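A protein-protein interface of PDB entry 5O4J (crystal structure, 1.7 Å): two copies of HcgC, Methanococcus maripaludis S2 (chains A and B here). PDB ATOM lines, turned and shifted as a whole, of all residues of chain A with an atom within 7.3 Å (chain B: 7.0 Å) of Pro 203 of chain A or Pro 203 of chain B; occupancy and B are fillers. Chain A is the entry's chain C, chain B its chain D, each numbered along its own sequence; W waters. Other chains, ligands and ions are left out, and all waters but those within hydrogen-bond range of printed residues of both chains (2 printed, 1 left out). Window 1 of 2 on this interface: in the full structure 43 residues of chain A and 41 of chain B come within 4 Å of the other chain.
The backbone carbonyl oxygen (O) of Pro 203 of chain A lies close to the backbone carbonyl oxygen (O) of Leu 205 of chain B, at 3.5 Å.
The backbone carbonyl oxygen of Leu 205 of chain A lies close to the backbone carbonyl oxygen of Leu 205 of chain B (3.4 Å).
SG of Cys 189 of chain A lies within hydrogen-bond range of O of Ile 185 of chain A (3.3 Å).
The backbone carbonyl oxygen of Thr 231 of chain A is in hydrogen-bond range of the backbone NH of Ile 202 of chain A.
O of Ala 229 of chain A sits at hydrogen-bond distance from N of Asn 204 of chain A.
The side-chain hydroxyl (OG1) of Thr 231 of chain A lies within hydrogen-bond range of the side-chain amide nitrogen (ND2) of Asn 204 of chain A (3.0 Å).
The backbone carbonyl oxygen (O) of Ile 185 of chain B is in hydrogen-bond range of the side-chain sulfur (SG) of Cys 189 of chain B.
N of Ile 202 of chain B lies within hydrogen-bond range of O of Thr 231 of chain B, 2.7 Å away.
Cys 189 of chain B touches Met 186 of chain A (CB to CE, 3.8 Å).
SD of Met 186 of chain A touches CG of Pro 203 of chain B (3.6 Å).
Met 186 of chain B touches Cys 189 of chain A (CE to CB, 3.7 Å).
O of Thr 201 of chain A touches CG1 of Val 182 of chain B, at 3.7 Å.
Ile 202 of chain A touches Val 182 of chain B (CD1 to CG2, 3.6 Å).
CG2 of Ile 202 of chain A touches N of Tyr 207 of chain B, at 3.95 Å.
Leu 205 of chain A touches Pro 203 of chain B.
Lys 206 of chain A touches Ile 202 of chain B (C to CG2, 3.5 Å).
Ile 202 of chain B touches Tyr 207 of chain A (CG2 to N, 3.96 Å).
Tyr 207 of chain A touches Thr 231 of chain B (CG to CG2, 3.9 Å).
Of chain B, only Met 186 (3.6 Å), Pro 203 (3.9 Å) and Leu 205 (3.5 Å) come within 4 Å of Pro 203 of chain A.
Of the printed residues of chain A, Leu 205 of chain B touches Pro 203 and Leu 205.
Of the printed residues of chain A, Val 182 of chain B touches Thr 201 (3.7 Å) and Ile 202 (3.6 Å).
Of the printed residues of chain A, Thr 231 of chain B touches Tyr 207 (3.9 Å).
Of the printed residues of chain A, Tyr 207 of chain B touches Ile 202 (3.95 Å).
Ile 230 of chain A touches none of the printed residues of chain B.
The nearest residue of chain B that does not touch Pro 203 of chain A is Lys 206 of chain B (4.7 Å).
The nearest residue of chain A that does not touch Pro 203 of chain B is Lys 206 of chain A (4.7 Å).
Along chain B the printed residues that touch a printed residue of chain A span positions 182 to 231.
Hydrophobic or aromatic side chains of chain A that line the printed part of chain B: Val 182, Met 186, Ile 202, Pro 203, Leu 205 and Tyr 207.
Among the printed residues, no Asp or Glu carboxylate lies within 4 Å of a Lys or Arg side-chain nitrogen of the other chain.
Val 182 of chain A touches Ile 202 of chain B, and with the chains exchanged Ile 202 of chain A touches Val 182 of chain B.
Ile 202 of chain A touches Tyr 207 of chain B, and with the chains exchanged Tyr 207 of chain A touches Ile 202 of chain B.
Pro 203 of chain A touches Leu 205 of chain B, and with the chains exchanged Leu 205 of chain A touches Pro 203 of chain B.
Leu 205 of chain A touches its own counterpart, Leu 205 of chain B.
Of the 19 pairs that touch across the chains among the printed residues, 17 have their exchanged pair printed and touching as well.
Water W1 lies within hydrogen-bond range of the side-chain amide oxygen (OD1) of Asn 204 of chain A (2.5 Å) and the backbone NH (N) of Tyr 207 of chain B (2.9 Å).
Water W2 lies within hydrogen-bond range of the side-chain amide oxygen of Asn 204 of chain B (2.6 Å) and the backbone NH of Tyr 207 of chain A (2.7 Å).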
ATOM      1  N   ILE A  18      -8.225  24.581   2.139  1.00  0.00           N
ATOM      2  CA  ILE A  18      -9.006  23.384   2.446  1.00  0.00           C
ATOM      3  C   ILE A  18      -9.864  23.613   3.683  1.00  0.00           C
ATOM      4  O   ILE A  18     -11.036  23.222   3.726  1.00  0.00           O
ATOM      5  CB  ILE A  18      -8.079  22.166   2.600  1.00  0.00           C
ATOM      6  CG1 ILE A  18      -7.278  21.958   1.309  1.00  0.00           C
ATOM      7  CG2 ILE A  18      -8.885  20.905   2.907  1.00  0.00           C
ATOM      8  CD1 ILE A  18      -6.003  21.204   1.506  1.00  0.00           C
ATOM      9  N   VAL A 182     -13.419  16.821  -0.727  1.00  0.00           N
ATOM     10  CA  VAL A 182     -12.660  16.224  -1.822  1.00  0.00           C
ATOM     11  C   VAL A 182     -13.379  16.439  -3.147  1.00  0.00           C
ATOM     12  O   VAL A 182     -12.775  16.842  -4.151  1.00  0.00           O
ATOM     13  CB  VAL A 182     -12.428  14.725  -1.549  1.00  0.00           C
ATOM     14  CG1 VAL A 182     -11.884  14.017  -2.780  1.00  0.00           C
ATOM     15  CG2 VAL A 182     -11.471  14.550  -0.349  1.00  0.00           C
ATOM     16  N   ILE A 185     -13.301  19.932  -4.499  1.00  0.00           N
ATOM     17  CA  ILE A 185     -11.992  20.276  -5.037  1.00  0.00           C
ATOM     18  C   ILE A 185     -11.773  19.584  -6.375  1.00  0.00           C
ATOM     19  O   ILE A 185     -11.299  20.200  -7.337  1.00  0.00           O
ATOM     20  CB  ILE A 185     -10.892  19.929  -4.018  1.00  0.00           C
ATOM     21  CG1 ILE A 185     -10.990  20.878  -2.817  1.00  0.00           C
ATOM     22  CG2 ILE A 185      -9.509  20.045  -4.645  1.00  0.00           C
ATOM     23  CD1 ILE A 185     -10.115  20.489  -1.653  1.00  0.00           C
ATOM     24  N   MET A 186     -12.142  18.307  -6.466  1.00  0.00           N
ATOM     25  CA  MET A 186     -11.941  17.564  -7.710  1.00  0.00           C
ATOM     26  C   MET A 186     -12.756  18.164  -8.848  1.00  0.00           C
ATOM     27  O   MET A 186     -12.255  18.312  -9.970  1.00  0.00           O
ATOM     28  CB  MET A 186     -12.301  16.094  -7.515  1.00  0.00           C
ATOM     29  CG  MET A 186     -11.345  15.326  -6.610  1.00  0.00           C
ATOM     30  SD  MET A 186      -9.658  15.250  -7.254  1.00  0.00           S
ATOM     31  CE  MET A 186      -9.817  14.054  -8.572  1.00  0.00           C
ATOM     32  N   CYS A 189     -11.189  21.481  -9.908  1.00  0.00           N
ATOM     33  CA  CYS A 189     -10.005  21.276 -10.739  1.00  0.00           C
ATOM     34  C   CYS A 189     -10.379  21.018 -12.186  1.00  0.00           C
ATOM     35  O   CYS A 189      -9.734  21.544 -13.102  1.00  0.00           O
ATOM     36  CB  CYS A 189      -9.179  20.101 -10.218  1.00  0.00           C
ATOM     37  SG  CYS A 189      -8.285  20.482  -8.739  1.00  0.00           S
ATOM     38  N   THR A 201      -3.598  21.551 -13.371  1.00  0.00           N
ATOM     39  CA  THR A 201      -4.307  22.005 -12.184  1.00  0.00           C
ATOM     40  C   THR A 201      -4.107  20.973 -11.086  1.00  0.00           C
ATOM     41  O   THR A 201      -4.463  19.805 -11.264  1.00  0.00           O
ATOM     42  CB  THR A 201      -5.797  22.195 -12.482  1.00  0.00           C
ATOM     43  OG1 THR A 201      -5.944  23.063 -13.610  1.00  0.00           O
ATOM     44  CG2 THR A 201      -6.510  22.807 -11.289  1.00  0.00           C
ATOM     45  N   ILE A 202      -3.557  21.406  -9.957  1.00  0.00           N
ATOM     46  CA  ILE A 202      -3.180  20.519  -8.858  1.00  0.00           C
ATOM     47  C   ILE A 202      -4.233  20.631  -7.755  1.00  0.00           C
ATOM     48  O   ILE A 202      -4.389  21.724  -7.182  1.00  0.00           O
ATOM     49  CB  ILE A 202      -1.796  20.874  -8.296  1.00  0.00           C
ATOM     50  CG1 ILE A 202      -0.706  20.692  -9.351  1.00  0.00           C
ATOM     51  CG2 ILE A 202      -1.499  20.052  -7.026  1.00  0.00           C
ATOM     52  CD1 ILE A 202      -0.434  19.253  -9.748  1.00  0.00           C
ATOM     53  N   PRO A 203      -4.924  19.548  -7.399  1.00  0.00           N
ATOM     54  CA  PRO A 203      -5.666  19.531  -6.130  1.00  0.00           C
ATOM     55  C   PRO A 203      -4.698  19.191  -5.008  1.00  0.00           C
ATOM     56  O   PRO A 203      -4.050  18.143  -5.036  1.00  0.00           O
ATOM     57  CB  PRO A 203      -6.698  18.419  -6.337  1.00  0.00           C
ATOM     58  CG  PRO A 203      -6.019  17.464  -7.260  1.00  0.00           C
ATOM     59  CD  PRO A 203      -4.998  18.241  -8.077  1.00  0.00           C
ATOM     60  N   ASN A 204      -4.600  20.069  -4.017  1.00  0.00           N
ATOM     61  CA  ASN A 204      -3.662  19.861  -2.917  1.00  0.00           C
ATOM     62  C   ASN A 204      -4.300  18.917  -1.898  1.00  0.00           C
ATOM     63  O   ASN A 204      -4.654  19.281  -0.776  1.00  0.00           O
ATOM     64  CB  ASN A 204      -3.264  21.194  -2.306  1.00  0.00           C
ATOM     65  CG  ASN A 204      -2.377  21.995  -3.226  1.00  0.00           C
ATOM     66  OD1 ASN A 204      -1.391  21.476  -3.746  1.00  0.00           O
ATOM     67  ND2 ASN A 204      -2.728  23.259  -3.449  1.00  0.00           N
ATOM     68  N   LEU A 205      -4.451  17.670  -2.321  1.00  0.00           N
ATOM     69  CA  LEU A 205      -5.145  16.668  -1.532  1.00  0.00           C
ATOM     70  C   LEU A 205      -4.165  15.624  -1.022  1.00  0.00           C
ATOM     71  O   LEU A 205      -3.088  15.410  -1.588  1.00  0.00           O
ATOM     72  CB  LEU A 205      -6.258  16.004  -2.352  1.00  0.00           C
ATOM     73  CG  LEU A 205      -7.426  16.931  -2.699  1.00  0.00           C
ATOM     74  CD1 LEU A 205      -8.367  16.255  -3.686  1.00  0.00           C
ATOM     75  CD2 LEU A 205      -8.193  17.347  -1.434  1.00  0.00           C
ATOM     76  N   LYS A 206      -4.546  15.008   0.089  1.00  0.00           N
ATOM     77  CA  LYS A 206      -3.851  13.862   0.651  1.00  0.00           C
ATOM     78  C   LYS A 206      -4.865  13.124   1.508  1.00  0.00           C
ATOM     79  O   LYS A 206      -6.015  13.550   1.645  1.00  0.00           O
ATOM     80  CB  LYS A 206      -2.617  14.282   1.455  1.00  0.00           C
ATOM     81  CG  LYS A 206      -2.917  15.148   2.666  1.00  0.00           C
ATOM     82  CD  LYS A 206      -1.692  15.283   3.567  1.00  0.00           C
ATOM     83  CE  LYS A 206      -1.453  14.009   4.368  1.00  0.00           C
ATOM     84  NZ  LYS A 206      -0.125  13.995   5.042  1.00  0.00           N
ATOM     85  N   TYR A 207      -4.447  11.996   2.075  1.00  0.00           N
ATOM     86  CA  TYR A 207      -5.351  11.194   2.895  1.00  0.00           C
ATOM     87  C   TYR A 207      -5.379  11.811   4.297  1.00  0.00           C
ATOM     88  O   TYR A 207      -4.806  11.301   5.258  1.00  0.00           O
ATOM     89  CB  TYR A 207      -4.916   9.734   2.883  1.00  0.00           C
ATOM     90  CG  TYR A 207      -5.752   8.805   3.740  1.00  0.00           C
ATOM     91  CD1 TYR A 207      -7.136   8.724   3.587  1.00  0.00           C
ATOM     92  CD2 TYR A 207      -5.148   8.000   4.700  1.00  0.00           C
ATOM     93  CE1 TYR A 207      -7.894   7.862   4.385  1.00  0.00           C
ATOM     94  CE2 TYR A 207      -5.893   7.145   5.487  1.00  0.00           C
ATOM     95  CZ  TYR A 207      -7.257   7.082   5.331  1.00  0.00           C
ATOM     96  OH  TYR A 207      -7.978   6.230   6.139  1.00  0.00           O
ATOM     97  N   SER A 228      -3.628  25.867   0.512  1.00  0.00           N
ATOM     98  CA  SER A 228      -4.473  26.234  -0.619  1.00  0.00           C
ATOM     99  C   SER A 228      -5.130  24.987  -1.195  1.00  0.00           C
ATOM    100  O   SER A 228      -4.493  23.940  -1.326  1.00  0.00           O
ATOM    101  CB  SER A 228      -3.648  26.929  -1.708  1.00  0.00           C
ATOM    102  OG  SER A 228      -3.179  28.196  -1.285  1.00  0.00           O
ATOM    103  N   ALA A 229      -6.417  25.098  -1.540  1.00  0.00           N
ATOM    104  CA  ALA A 229      -7.120  23.943  -2.097  1.00  0.00           C
ATOM    105  C   ALA A 229      -6.539  23.532  -3.438  1.00  0.00           C
ATOM    106  O   ALA A 229      -6.445  22.333  -3.742  1.00  0.00           O
ATOM    107  CB  ALA A 229      -8.607  24.247  -2.252  1.00  0.00           C
ATOM    108  N   ILE A 230      -6.168  24.507  -4.263  1.00  0.00           N
ATOM    109  CA  ILE A 230      -5.769  24.249  -5.640  1.00  0.00           C
ATOM    110  C   ILE A 230      -4.577  25.124  -5.988  1.00  0.00           C
ATOM    111  O   ILE A 230      -4.511  26.294  -5.594  1.00  0.00           O
ATOM    112  CB  ILE A 230      -6.938  24.496  -6.618  1.00  0.00           C
ATOM    113  CG1 ILE A 230      -8.043  23.459  -6.369  1.00  0.00           C
ATOM    114  CG2 ILE A 230      -6.458  24.448  -8.065  1.00  0.00           C
ATOM    115  CD1 ILE A 230      -9.306  23.690  -7.151  1.00  0.00           C
ATOM    116  N   THR A 231      -3.636  24.545  -6.729  1.00  0.00           N
ATOM    117  CA  THR A 231      -2.518  25.273  -7.315  1.00  0.00           C
ATOM    118  C   THR A 231      -2.572  25.084  -8.824  1.00  0.00           C
ATOM    119  O   THR A 231      -2.709  23.955  -9.304  1.00  0.00           O
ATOM    120  CB  THR A 231      -1.183  24.779  -6.752  1.00  0.00           C
ATOM    121  OG1 THR A 231      -1.175  24.959  -5.330  1.00  0.00           O
ATOM    122  CG2 THR A 231      -0.021  25.547  -7.366  1.00  0.00           C
ATOM    123  N   ILE B  18       3.647   7.493  -7.936  1.00  0.00           N
ATOM    124  CA  ILE B  18       3.766   8.602  -8.882  1.00  0.00           C
ATOM    125  C   ILE B  18       5.004   8.431  -9.753  1.00  0.00           C
ATOM    126  O   ILE B  18       4.967   8.670 -10.967  1.00  0.00           O
ATOM    127  CB  ILE B  18       3.764   9.954  -8.144  1.00  0.00           C
ATOM    128  CG1 ILE B  18       2.474  10.118  -7.334  1.00  0.00           C
ATOM    129  CG2 ILE B  18       3.886  11.102  -9.144  1.00  0.00           C
ATOM    130  CD1 ILE B  18       2.590  11.090  -6.200  1.00  0.00           C
ATOM    131  N   VAL B 182      -0.230  14.202 -13.957  1.00  0.00           N
ATOM    132  CA  VAL B 182      -1.364  14.772 -13.238  1.00  0.00           C
ATOM    133  C   VAL B 182      -2.673  14.329 -13.878  1.00  0.00           C
ATOM    134  O   VAL B 182      -3.597  13.885 -13.193  1.00  0.00           O
ATOM    135  CB  VAL B 182      -1.240  16.306 -13.175  1.00  0.00           C
ATOM    136  CG1 VAL B 182      -2.526  16.943 -12.672  1.00  0.00           C
ATOM    137  CG2 VAL B 182      -0.083  16.693 -12.279  1.00  0.00           C
ATOM    138  N   ILE B 185      -3.589  10.683 -13.337  1.00  0.00           N
ATOM    139  CA  ILE B 185      -4.066  10.437 -11.986  1.00  0.00           C
ATOM    140  C   ILE B 185      -5.474  10.994 -11.806  1.00  0.00           C
ATOM    141  O   ILE B 185      -6.345  10.325 -11.242  1.00  0.00           O
ATOM    142  CB  ILE B 185      -3.057  11.014 -10.971  1.00  0.00           C
ATOM    143  CG1 ILE B 185      -1.784  10.156 -10.985  1.00  0.00           C
ATOM    144  CG2 ILE B 185      -3.649  11.075  -9.578  1.00  0.00           C
ATOM    145  CD1 ILE B 185      -0.594  10.740 -10.216  1.00  0.00           C
ATOM    146  N   MET B 186      -5.733  12.206 -12.313  1.00  0.00           N
ATOM    147  CA  MET B 186      -7.048  12.817 -12.135  1.00  0.00           C
ATOM    148  C   MET B 186      -8.132  12.007 -12.834  1.00  0.00           C
ATOM    149  O   MET B 186      -9.188  11.730 -12.249  1.00  0.00           O
ATOM    150  CB  MET B 186      -7.028  14.258 -12.649  1.00  0.00           C
ATOM    151  CG  MET B 186      -6.159  15.194 -11.829  1.00  0.00           C
ATOM    152  SD  MET B 186      -6.741  15.398 -10.136  1.00  0.00           S
ATOM    153  CE  MET B 186      -8.112  16.516 -10.404  1.00  0.00           C
ATOM    154  N   CYS B 189      -8.741   8.831 -10.939  1.00  0.00           N
ATOM    155  CA  CYS B 189      -9.524   9.086  -9.735  1.00  0.00           C
ATOM    156  C   CYS B 189     -11.007   9.144 -10.037  1.00  0.00           C
ATOM    157  O   CYS B 189     -11.816   8.579  -9.298  1.00  0.00           O
ATOM    158  CB  CYS B 189      -9.099  10.395  -9.089  1.00  0.00           C
ATOM    159  SG  CYS B 189      -7.643  10.244  -8.134  1.00  0.00           S
ATOM    160  N   THR B 201     -11.997   9.285  -3.224  1.00  0.00           N
ATOM    161  CA  THR B 201     -10.784   8.878  -3.919  1.00  0.00           C
ATOM    162  C   THR B 201      -9.808  10.042  -3.889  1.00  0.00           C
ATOM    163  O   THR B 201     -10.138  11.134  -4.361  1.00  0.00           O
ATOM    164  CB  THR B 201     -11.113   8.470  -5.358  1.00  0.00           C
ATOM    165  OG1 THR B 201     -12.155   7.484  -5.352  1.00  0.00           O
ATOM    166  CG2 THR B 201      -9.898   7.867  -6.044  1.00  0.00           C
ATOM    167  N   ILE B 202      -8.624   9.826  -3.330  1.00  0.00           N
ATOM    168  CA  ILE B 202      -7.645  10.892  -3.128  1.00  0.00           C
ATOM    169  C   ILE B 202      -6.570  10.777  -4.204  1.00  0.00           C
ATOM    170  O   ILE B 202      -5.880   9.750  -4.262  1.00  0.00           O
ATOM    171  CB  ILE B 202      -7.003  10.821  -1.737  1.00  0.00           C
ATOM    172  CG1 ILE B 202      -8.051  11.000  -0.645  1.00  0.00           C
ATOM    173  CG2 ILE B 202      -5.875  11.873  -1.612  1.00  0.00           C
ATOM    174  CD1 ILE B 202      -8.631  12.388  -0.565  1.00  0.00           C
ATOM    175  N   PRO B 203      -6.368  11.801  -5.038  1.00  0.00           N
ATOM    176  CA  PRO B 203      -5.126  11.873  -5.817  1.00  0.00           C
ATOM    177  C   PRO B 203      -4.031  12.448  -4.930  1.00  0.00           C
ATOM    178  O   PRO B 203      -4.177  13.542  -4.381  1.00  0.00           O
ATOM    179  CB  PRO B 203      -5.487  12.823  -6.965  1.00  0.00           C
ATOM    180  CG  PRO B 203      -6.517  13.739  -6.372  1.00  0.00           C
ATOM    181  CD  PRO B 203      -7.211  12.994  -5.244  1.00  0.00           C
ATOM    182  N   ASN B 204      -2.936  11.706  -4.773  1.00  0.00           N
ATOM    183  CA  ASN B 204      -1.858  12.128  -3.876  1.00  0.00           C
ATOM    184  C   ASN B 204      -0.942  13.106  -4.615  1.00  0.00           C
ATOM    185  O   ASN B 204       0.216  12.827  -4.935  1.00  0.00           O
ATOM    186  CB  ASN B 204      -1.104  10.917  -3.348  1.00  0.00           C
ATOM    187  CG  ASN B 204      -1.928  10.116  -2.366  1.00  0.00           C
ATOM    188  OD1 ASN B 204      -2.501  10.672  -1.433  1.00  0.00           O
ATOM    189  ND2 ASN B 204      -2.000   8.808  -2.574  1.00  0.00           N
ATOM    190  N   LEU B 205      -1.495  14.284  -4.888  1.00  0.00           N
ATOM    191  CA  LEU B 205      -0.833  15.291  -5.702  1.00  0.00           C
ATOM    192  C   LEU B 205      -0.443  16.510  -4.879  1.00  0.00           C
ATOM    193  O   LEU B 205      -1.042  16.816  -3.844  1.00  0.00           O
ATOM    194  CB  LEU B 205      -1.733  15.733  -6.867  1.00  0.00           C
ATOM    195  CG  LEU B 205      -2.004  14.671  -7.937  1.00  0.00           C
ATOM    196  CD1 LEU B 205      -3.038  15.171  -8.936  1.00  0.00           C
ATOM    197  CD2 LEU B 205      -0.713  14.288  -8.631  1.00  0.00           C
ATOM    198  N   LYS B 206       0.580  17.201  -5.369  1.00  0.00           N
ATOM    199  CA  LYS B 206       1.002  18.494  -4.855  1.00  0.00           C
ATOM    200  C   LYS B 206       1.770  19.188  -5.974  1.00  0.00           C
ATOM    201  O   LYS B 206       1.963  18.630  -7.057  1.00  0.00           O
ATOM    202  CB  LYS B 206       1.851  18.351  -3.587  1.00  0.00           C
ATOM    203  CG  LYS B 206       3.150  17.577  -3.795  1.00  0.00           C
ATOM    204  CD  LYS B 206       4.084  17.702  -2.600  1.00  0.00           C
ATOM    205  CE  LYS B 206       4.767  19.063  -2.552  1.00  0.00           C
ATOM    206  NZ  LYS B 206       5.472  19.272  -1.254  1.00  0.00           N
ATOM    207  N   TYR B 207       2.209  20.417  -5.709  1.00  0.00           N
ATOM    208  CA  TYR B 207       2.934  21.192  -6.714  1.00  0.00           C
ATOM    209  C   TYR B 207       4.396  20.740  -6.697  1.00  0.00           C
ATOM    210  O   TYR B 207       5.292  21.420  -6.192  1.00  0.00           O
ATOM    211  CB  TYR B 207       2.777  22.683  -6.445  1.00  0.00           C
ATOM    212  CG  TYR B 207       3.501  23.591  -7.424  1.00  0.00           C
ATOM    213  CD1 TYR B 207       3.291  23.488  -8.796  1.00  0.00           C
ATOM    214  CD2 TYR B 207       4.377  24.570  -6.966  1.00  0.00           C
ATOM    215  CE1 TYR B 207       3.951  24.327  -9.685  1.00  0.00           C
ATOM    216  CE2 TYR B 207       5.037  25.404  -7.842  1.00  0.00           C
ATOM    217  CZ  TYR B 207       4.824  25.283  -9.196  1.00  0.00           C
ATOM    218  OH  TYR B 207       5.495  26.124 -10.060  1.00  0.00           O
ATOM    219  N   SER B 228       2.241   6.553  -3.265  1.00  0.00           N
ATOM    220  CA  SER B 228       1.143   5.961  -4.023  1.00  0.00           C
ATOM    221  C   SER B 228       0.428   7.052  -4.805  1.00  0.00           C
ATOM    222  O   SER B 228       0.184   8.142  -4.287  1.00  0.00           O
ATOM    223  CB  SER B 228       0.140   5.255  -3.102  1.00  0.00           C
ATOM    224  OG  SER B 228       0.690   4.093  -2.502  1.00  0.00           O
ATOM    225  N   ALA B 229       0.095   6.753  -6.057  1.00  0.00           N
ATOM    226  CA  ALA B 229      -0.598   7.735  -6.877  1.00  0.00           C
ATOM    227  C   ALA B 229      -1.969   8.069  -6.297  1.00  0.00           C
ATOM    228  O   ALA B 229      -2.398   9.227  -6.333  1.00  0.00           O
ATOM    229  CB  ALA B 229      -0.728   7.219  -8.308  1.00  0.00           C
ATOM    230  N   ILE B 230      -2.672   7.074  -5.760  1.00  0.00           N
ATOM    231  CA  ILE B 230      -4.062   7.239  -5.339  1.00  0.00           C
ATOM    232  C   ILE B 230      -4.293   6.493  -4.030  1.00  0.00           C
ATOM    233  O   ILE B 230      -3.770   5.393  -3.815  1.00  0.00           O
ATOM    234  CB  ILE B 230      -5.048   6.758  -6.429  1.00  0.00           C
ATOM    235  CG1 ILE B 230      -4.926   7.650  -7.669  1.00  0.00           C
ATOM    236  CG2 ILE B 230      -6.496   6.777  -5.892  1.00  0.00           C
ATOM    237  CD1 ILE B 230      -5.711   7.180  -8.865  1.00  0.00           C
ATOM    238  N   THR B 231      -5.082   7.104  -3.152  1.00  0.00           N
ATOM    239  CA  THR B 231      -5.566   6.462  -1.941  1.00  0.00           C
ATOM    240  C   THR B 231      -7.086   6.478  -1.970  1.00  0.00           C
ATOM    241  O   THR B 231      -7.691   7.527  -2.219  1.00  0.00           O
ATOM    242  CB  THR B 231      -5.033   7.170  -0.698  1.00  0.00           C
ATOM    243  OG1 THR B 231      -3.601   7.134  -0.720  1.00  0.00           O
ATOM    244  CG2 THR B 231      -5.559   6.498   0.585  1.00  0.00           C
HETATM  245  O   HOH W   1       1.081  21.976  -3.509  1.00  0.00           O
HETATM  246  O   HOH W   2      -2.188  10.861   1.143  1.00  0.00           O
